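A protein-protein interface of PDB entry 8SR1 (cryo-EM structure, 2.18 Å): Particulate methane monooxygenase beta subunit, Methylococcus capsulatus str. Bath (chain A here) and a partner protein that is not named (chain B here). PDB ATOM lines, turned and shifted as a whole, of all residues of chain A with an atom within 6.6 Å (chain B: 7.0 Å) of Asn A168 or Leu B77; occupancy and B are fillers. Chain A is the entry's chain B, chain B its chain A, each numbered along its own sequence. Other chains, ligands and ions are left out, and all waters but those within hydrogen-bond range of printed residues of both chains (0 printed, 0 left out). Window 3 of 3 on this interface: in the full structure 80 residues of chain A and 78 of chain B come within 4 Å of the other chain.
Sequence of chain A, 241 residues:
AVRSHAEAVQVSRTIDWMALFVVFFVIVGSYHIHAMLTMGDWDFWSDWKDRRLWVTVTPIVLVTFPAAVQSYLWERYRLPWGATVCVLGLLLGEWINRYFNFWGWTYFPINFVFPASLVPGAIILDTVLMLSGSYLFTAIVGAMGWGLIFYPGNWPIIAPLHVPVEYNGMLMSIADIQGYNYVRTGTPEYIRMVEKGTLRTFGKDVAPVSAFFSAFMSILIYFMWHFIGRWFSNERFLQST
CD2 of Leu B77 touches O of Tyr A167 (3.98 Å). Asn A168 touches Lys B69 (OD1 to O, 3.98 Å). OD1 of Asn A168 touches CG of Glu B70 (3.5 Å). Asn A168 touches Leu B77 (CB to CD1, 3.9 Å). Met A170 touches Pro B79 (SD to CD, 3.6 Å). CE of Met A170 touches NH2 of Arg B80, at 3.3 Å. Pro B79 touches Met A172 (CB to CE, 3.8 Å). Lys B69 touches Tyr A180 (O to CE2, 3.4 Å). OH of Tyr A180 touches C of Glu B70 (3.1 Å). Pro B79 touches Tyr A180 (CA to CE1, 3.5 Å).
Printed residues of chain A that touch a printed residue of chain B: Tyr A167, Asn A168, Met A170, Met A172 and Tyr A180. Among the printed residues, no Asp or Glu carboxylate lies within 4 Å of a Lys or Arg side-chain nitrogen of the other chain.
The side-chain hydroxyl (OH) of Tyr A167 is in hydrogen-bond range of the backbone carbonyl oxygen (O) of Lys B69 (2.7 Å). OH of Tyr A180 is in hydrogen-bond range of N of Ser B71.
OE1 of Glu B70 sits at hydrogen-bond distance from OH of Tyr B72 (3.2 Å). O of Ser B71 sits at hydrogen-bond distance from N of Val B78 (2.9 Å). OE2 of Glu A166 sits at hydrogen-bond distance from N of Met A170, at 3.3 Å.
Printed residues of chain B within 4 Å of Asn A168: Lys B69 (3.98 Å), Glu B70 (3.5 Å) and Leu B77 (3.9 Å). Of the printed residues of chain A, Leu B77 touches Tyr A167 (3.98 Å), Asn A168 (3.9 Å) and Tyr A180 (3.9 Å). Of the printed residues of chain B, Met A172 touches Pro B79 (3.8 Å). Printed residues of chain B within 4 Å of Tyr A167: Lys B69 and Leu B77. Met B237 touches none of the printed residues of chain A. The nearest printed residue of chain A that does not touch Leu B77 is Met A170 (4.2 Å).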
ATOM      1  N   GLU A 166       5.089 -23.701 -10.317  1.00  0.00           N
ATOM      2  CA  GLU A 166       3.925 -24.056 -11.125  1.00  0.00           C
ATOM      3  C   GLU A 166       3.026 -24.932 -10.262  1.00  0.00           C
ATOM      4  O   GLU A 166       3.274 -26.129 -10.103  1.00  0.00           O
ATOM      5  CB  GLU A 166       4.366 -24.773 -12.395  1.00  0.00           C
ATOM      6  CG  GLU A 166       3.405 -24.661 -13.555  1.00  0.00           C
ATOM      7  CD  GLU A 166       2.058 -25.257 -13.258  1.00  0.00           C
ATOM      8  OE1 GLU A 166       1.981 -26.476 -12.991  1.00  0.00           O
ATOM      9  OE2 GLU A 166       1.074 -24.496 -13.277  1.00  0.00           O
ATOM     10  N   TYR A 167       1.978 -24.343  -9.697  1.00  0.00           N
ATOM     11  CA  TYR A 167       1.143 -25.011  -8.696  1.00  0.00           C
ATOM     12  C   TYR A 167      -0.249 -25.245  -9.273  1.00  0.00           C
ATOM     13  O   TYR A 167      -1.073 -24.328  -9.311  1.00  0.00           O
ATOM     14  CB  TYR A 167       1.078 -24.187  -7.412  1.00  0.00           C
ATOM     15  CG  TYR A 167       0.556 -24.950  -6.217  1.00  0.00           C
ATOM     16  CD1 TYR A 167       1.383 -25.799  -5.496  1.00  0.00           C
ATOM     17  CD2 TYR A 167      -0.764 -24.815  -5.807  1.00  0.00           C
ATOM     18  CE1 TYR A 167       0.910 -26.495  -4.402  1.00  0.00           C
ATOM     19  CE2 TYR A 167      -1.244 -25.508  -4.714  1.00  0.00           C
ATOM     20  CZ  TYR A 167      -0.403 -26.345  -4.016  1.00  0.00           C
ATOM     21  OH  TYR A 167      -0.881 -27.038  -2.928  1.00  0.00           O
ATOM     22  N   ASN A 168      -0.503 -26.483  -9.705  1.00  0.00           N
ATOM     23  CA  ASN A 168      -1.826 -26.916 -10.166  1.00  0.00           C
ATOM     24  C   ASN A 168      -2.376 -26.005 -11.263  1.00  0.00           C
ATOM     25  O   ASN A 168      -3.540 -25.605 -11.244  1.00  0.00           O
ATOM     26  CB  ASN A 168      -2.806 -27.008  -8.995  1.00  0.00           C
ATOM     27  CG  ASN A 168      -2.424 -28.087  -8.002  1.00  0.00           C
ATOM     28  OD1 ASN A 168      -2.071 -27.797  -6.859  1.00  0.00           O
ATOM     29  ND2 ASN A 168      -2.497 -29.340  -8.431  1.00  0.00           N
ATOM     30  N   GLY A 169      -1.525 -25.674 -12.231  1.00  0.00           N
ATOM     31  CA  GLY A 169      -1.933 -24.885 -13.372  1.00  0.00           C
ATOM     32  C   GLY A 169      -1.780 -23.387 -13.215  1.00  0.00           C
ATOM     33  O   GLY A 169      -1.909 -22.661 -14.208  1.00  0.00           O
ATOM     34  N   MET A 170      -1.503 -22.900 -12.010  1.00  0.00           N
ATOM     35  CA  MET A 170      -1.382 -21.474 -11.747  1.00  0.00           C
ATOM     36  C   MET A 170       0.018 -21.157 -11.242  1.00  0.00           C
ATOM     37  O   MET A 170       0.632 -21.963 -10.535  1.00  0.00           O
ATOM     38  CB  MET A 170      -2.426 -21.017 -10.724  1.00  0.00           C
ATOM     39  CG  MET A 170      -3.810 -20.793 -11.317  1.00  0.00           C
ATOM     40  SD  MET A 170      -4.859 -19.720 -10.315  1.00  0.00           S
ATOM     41  CE  MET A 170      -4.018 -18.154 -10.497  1.00  0.00           C
ATOM     42  N   MET A 172       2.518 -19.478  -8.813  1.00  0.00           N
ATOM     43  CA  MET A 172       2.492 -19.038  -7.427  1.00  0.00           C
ATOM     44  C   MET A 172       3.912 -18.997  -6.889  1.00  0.00           C
ATOM     45  O   MET A 172       4.747 -19.839  -7.231  1.00  0.00           O
ATOM     46  CB  MET A 172       1.630 -19.964  -6.556  1.00  0.00           C
ATOM     47  CG  MET A 172       0.133 -19.755  -6.706  1.00  0.00           C
ATOM     48  SD  MET A 172      -0.830 -21.029  -5.871  1.00  0.00           S
ATOM     49  CE  MET A 172      -0.942 -20.342  -4.220  1.00  0.00           C
ATOM     50  N   TYR A 180      -1.581 -20.360   0.964  1.00  0.00           N
ATOM     51  CA  TYR A 180      -2.653 -21.221   0.479  1.00  0.00           C
ATOM     52  C   TYR A 180      -2.788 -22.484   1.319  1.00  0.00           C
ATOM     53  O   TYR A 180      -3.894 -22.846   1.738  1.00  0.00           O
ATOM     54  CB  TYR A 180      -2.397 -21.575  -0.983  1.00  0.00           C
ATOM     55  CG  TYR A 180      -3.527 -22.304  -1.662  1.00  0.00           C
ATOM     56  CD1 TYR A 180      -4.824 -21.819  -1.609  1.00  0.00           C
ATOM     57  CD2 TYR A 180      -3.292 -23.474  -2.369  1.00  0.00           C
ATOM     58  CE1 TYR A 180      -5.857 -22.486  -2.232  1.00  0.00           C
ATOM     59  CE2 TYR A 180      -4.316 -24.146  -2.995  1.00  0.00           C
ATOM     60  CZ  TYR A 180      -5.596 -23.647  -2.926  1.00  0.00           C
ATOM     61  OH  TYR A 180      -6.615 -24.317  -3.554  1.00  0.00           O
ATOM     62  N   LYS B  69      -4.426 -28.462   0.053  1.00  0.00           N
ATOM     63  CA  LYS B  69      -3.658 -28.784  -1.145  1.00  0.00           C
ATOM     64  C   LYS B  69      -4.266 -28.122  -2.373  1.00  0.00           C
ATOM     65  O   LYS B  69      -3.562 -27.498  -3.176  1.00  0.00           O
ATOM     66  CB  LYS B  69      -3.581 -30.301  -1.326  1.00  0.00           C
ATOM     67  CG  LYS B  69      -2.412 -30.954  -0.606  1.00  0.00           C
ATOM     68  CD  LYS B  69      -1.106 -30.230  -0.886  1.00  0.00           C
ATOM     69  CE  LYS B  69      -0.664 -30.411  -2.328  1.00  0.00           C
ATOM     70  NZ  LYS B  69       0.739 -29.967  -2.544  1.00  0.00           N
ATOM     71  N   GLU B  70      -5.584 -28.235  -2.530  1.00  0.00           N
ATOM     72  CA  GLU B  70      -6.276 -27.664  -3.674  1.00  0.00           C
ATOM     73  C   GLU B  70      -7.668 -27.222  -3.247  1.00  0.00           C
ATOM     74  O   GLU B  70      -8.236 -27.733  -2.278  1.00  0.00           O
ATOM     75  CB  GLU B  70      -6.381 -28.662  -4.831  1.00  0.00           C
ATOM     76  CG  GLU B  70      -5.073 -28.982  -5.529  1.00  0.00           C
ATOM     77  CD  GLU B  70      -4.863 -30.469  -5.710  1.00  0.00           C
ATOM     78  OE1 GLU B  70      -5.802 -31.151  -6.170  1.00  0.00           O
ATOM     79  OE2 GLU B  70      -3.758 -30.959  -5.395  1.00  0.00           O
ATOM     80  N   SER B  71      -8.212 -26.268  -3.991  1.00  0.00           N
ATOM     81  CA  SER B  71      -9.590 -25.830  -3.815  1.00  0.00           C
ATOM     82  C   SER B  71     -10.118 -25.397  -5.173  1.00  0.00           C
ATOM     83  O   SER B  71      -9.410 -24.720  -5.924  1.00  0.00           O
ATOM     84  CB  SER B  71      -9.698 -24.683  -2.804  1.00  0.00           C
ATOM     85  OG  SER B  71      -8.791 -23.642  -3.115  1.00  0.00           O
ATOM     86  N   TYR B  72     -11.347 -25.793  -5.489  1.00  0.00           N
ATOM     87  CA  TYR B  72     -11.937 -25.522  -6.789  1.00  0.00           C
ATOM     88  C   TYR B  72     -13.331 -24.942  -6.625  1.00  0.00           C
ATOM     89  O   TYR B  72     -14.088 -25.355  -5.744  1.00  0.00           O
ATOM     90  CB  TYR B  72     -12.016 -26.793  -7.648  1.00  0.00           C
ATOM     91  CG  TYR B  72     -10.689 -27.477  -7.873  1.00  0.00           C
ATOM     92  CD1 TYR B  72     -10.188 -28.379  -6.948  1.00  0.00           C
ATOM     93  CD2 TYR B  72      -9.938 -27.218  -9.008  1.00  0.00           C
ATOM     94  CE1 TYR B  72      -8.979 -29.006  -7.148  1.00  0.00           C
ATOM     95  CE2 TYR B  72      -8.723 -27.840  -9.217  1.00  0.00           C
ATOM     96  CZ  TYR B  72      -8.249 -28.733  -8.282  1.00  0.00           C
ATOM     97  OH  TYR B  72      -7.042 -29.356  -8.483  1.00  0.00           O
ATOM     98  N   ILE B  73     -13.658 -23.973  -7.473  1.00  0.00           N
ATOM     99  CA  ILE B  73     -15.026 -23.509  -7.662  1.00  0.00           C
ATOM    100  C   ILE B  73     -15.364 -23.729  -9.128  1.00  0.00           C
ATOM    101  O   ILE B  73     -14.696 -23.182 -10.015  1.00  0.00           O
ATOM    102  CB  ILE B  73     -15.197 -22.035  -7.264  1.00  0.00           C
ATOM    103  CG1 ILE B  73     -14.923 -21.854  -5.768  1.00  0.00           C
ATOM    104  CG2 ILE B  73     -16.591 -21.546  -7.633  1.00  0.00           C
ATOM    105  CD1 ILE B  73     -15.486 -20.576  -5.188  1.00  0.00           C
ATOM    106  N   GLY B  75     -14.701 -25.991 -11.776  1.00  0.00           N
ATOM    107  CA  GLY B  75     -13.742 -27.048 -12.011  1.00  0.00           C
ATOM    108  C   GLY B  75     -12.317 -26.534 -12.026  1.00  0.00           C
ATOM    109  O   GLY B  75     -11.386 -27.264 -12.371  1.00  0.00           O
ATOM    110  N   GLN B  76     -12.141 -25.272 -11.646  1.00  0.00           N
ATOM    111  CA  GLN B  76     -10.866 -24.582 -11.759  1.00  0.00           C
ATOM    112  C   GLN B  76     -10.344 -24.177 -10.385  1.00  0.00           C
ATOM    113  O   GLN B  76     -11.119 -23.839  -9.487  1.00  0.00           O
ATOM    114  CB  GLN B  76     -11.003 -23.362 -12.668  1.00  0.00           C
ATOM    115  CG  GLN B  76     -11.956 -22.310 -12.150  1.00  0.00           C
ATOM    116  CD  GLN B  76     -11.456 -20.909 -12.400  1.00  0.00           C
ATOM    117  OE1 GLN B  76     -10.586 -20.417 -11.686  1.00  0.00           O
ATOM    118  NE2 GLN B  76     -12.000 -20.257 -13.420  1.00  0.00           N
ATOM    119  N   LEU B  77      -9.020 -24.217 -10.236  1.00  0.00           N
ATOM    120  CA  LEU B  77      -8.390 -23.942  -8.951  1.00  0.00           C
ATOM    121  C   LEU B  77      -8.573 -22.484  -8.554  1.00  0.00           C
ATOM    122  O   LEU B  77      -8.493 -21.579  -9.390  1.00  0.00           O
ATOM    123  CB  LEU B  77      -6.902 -24.295  -9.018  1.00  0.00           C
ATOM    124  CG  LEU B  77      -6.133 -24.313  -7.700  1.00  0.00           C
ATOM    125  CD1 LEU B  77      -6.050 -25.727  -7.154  1.00  0.00           C
ATOM    126  CD2 LEU B  77      -4.746 -23.728  -7.889  1.00  0.00           C
ATOM    127  N   VAL B  78      -8.811 -22.256  -7.267  1.00  0.00           N
ATOM    128  CA  VAL B  78      -9.100 -20.913  -6.769  1.00  0.00           C
ATOM    129  C   VAL B  78      -8.202 -20.583  -5.580  1.00  0.00           C
ATOM    130  O   VAL B  78      -8.687 -20.474  -4.446  1.00  0.00           O
ATOM    131  CB  VAL B  78     -10.588 -20.772  -6.410  1.00  0.00           C
ATOM    132  CG1 VAL B  78     -11.415 -20.653  -7.672  1.00  0.00           C
ATOM    133  CG2 VAL B  78     -11.065 -21.968  -5.598  1.00  0.00           C
ATOM    134  N   PRO B  79      -6.893 -20.396  -5.786  1.00  0.00           N
ATOM    135  CA  PRO B  79      -6.027 -20.014  -4.662  1.00  0.00           C
ATOM    136  C   PRO B  79      -6.200 -18.569  -4.228  1.00  0.00           C
ATOM    137  O   PRO B  79      -5.667 -18.192  -3.176  1.00  0.00           O
ATOM    138  CB  PRO B  79      -4.619 -20.260  -5.208  1.00  0.00           C
ATOM    139  CG  PRO B  79      -4.758 -20.019  -6.666  1.00  0.00           C
ATOM    140  CD  PRO B  79      -6.146 -20.466  -7.053  1.00  0.00           C
ATOM    141  N   ARG B  80      -6.914 -17.759  -4.995  1.00  0.00           N
ATOM    142  CA  ARG B  80      -7.148 -16.358  -4.689  1.00  0.00           C
ATOM    143  C   ARG B  80      -8.636 -16.128  -4.448  1.00  0.00           C
ATOM    144  O   ARG B  80      -9.459 -17.041  -4.554  1.00  0.00           O
ATOM    145  CB  ARG B  80      -6.628 -15.469  -5.818  1.00  0.00           C
ATOM    146  CG  ARG B  80      -5.300 -15.922  -6.402  1.00  0.00           C
ATOM    147  CD  ARG B  80      -4.537 -14.755  -6.990  1.00  0.00           C
ATOM    148  NE  ARG B  80      -3.809 -15.118  -8.199  1.00  0.00           N
ATOM    149  CZ  ARG B  80      -3.983 -14.535  -9.378  1.00  0.00           C
ATOM    150  NH1 ARG B  80      -4.871 -13.573  -9.547  1.00  0.00           N
ATOM    151  NH2 ARG B  80      -3.241 -14.927 -10.408  1.00  0.00           N
ATOM    152  N   VAL B  82     -12.393 -14.844  -5.250  1.00  0.00           N
ATOM    153  CA  VAL B  82     -13.188 -15.023  -6.457  1.00  0.00           C
ATOM    154  C   VAL B  82     -14.440 -14.164  -6.368  1.00  0.00           C
ATOM    155  O   VAL B  82     -14.840 -13.708  -5.294  1.00  0.00           O
ATOM    156  CB  VAL B  82     -13.565 -16.498  -6.694  1.00  0.00           C
ATOM    157  CG1 VAL B  82     -12.321 -17.359  -6.737  1.00  0.00           C
ATOM    158  CG2 VAL B  82     -14.520 -16.983  -5.621  1.00  0.00           C
ATOM    159  N   MET B 237     -10.280 -13.286  -8.789  1.00  0.00           N
ATOM    160  CA  MET B 237     -10.432 -14.011 -10.042  1.00  0.00           C
ATOM    161  C   MET B 237     -11.899 -13.985 -10.457  1.00  0.00           C
ATOM    162  O   MET B 237     -12.772 -14.427  -9.704  1.00  0.00           O
ATOM    163  CB  MET B 237      -9.936 -15.446  -9.890  1.00  0.00           C
ATOM    164  CG  MET B 237      -8.421 -15.558  -9.849  1.00  0.00           C
ATOM    165  SD  MET B 237      -7.851 -17.193  -9.355  1.00  0.00           S
ATOM    166  CE  MET B 237      -8.735 -18.210 -10.525  1.00  0.00           C
ATOM    167  N   MET B 240     -16.060 -17.141 -12.574  1.00  0.00           N
ATOM    168  CA  MET B 240     -16.372 -18.426 -11.960  1.00  0.00           C
ATOM    169  C   MET B 240     -17.553 -19.033 -12.703  1.00  0.00           C
ATOM    170  O   MET B 240     -18.560 -18.359 -12.930  1.00  0.00           O
ATOM    171  CB  MET B 240     -16.680 -18.261 -10.474  1.00  0.00           C
ATOM    172  CG  MET B 240     -15.544 -17.689  -9.639  1.00  0.00           C
ATOM    173  SD  MET B 240     -14.100 -18.767  -9.531  1.00  0.00           S
ATOM    174  CE  MET B 240     -13.056 -18.110 -10.830  1.00  0.00           C
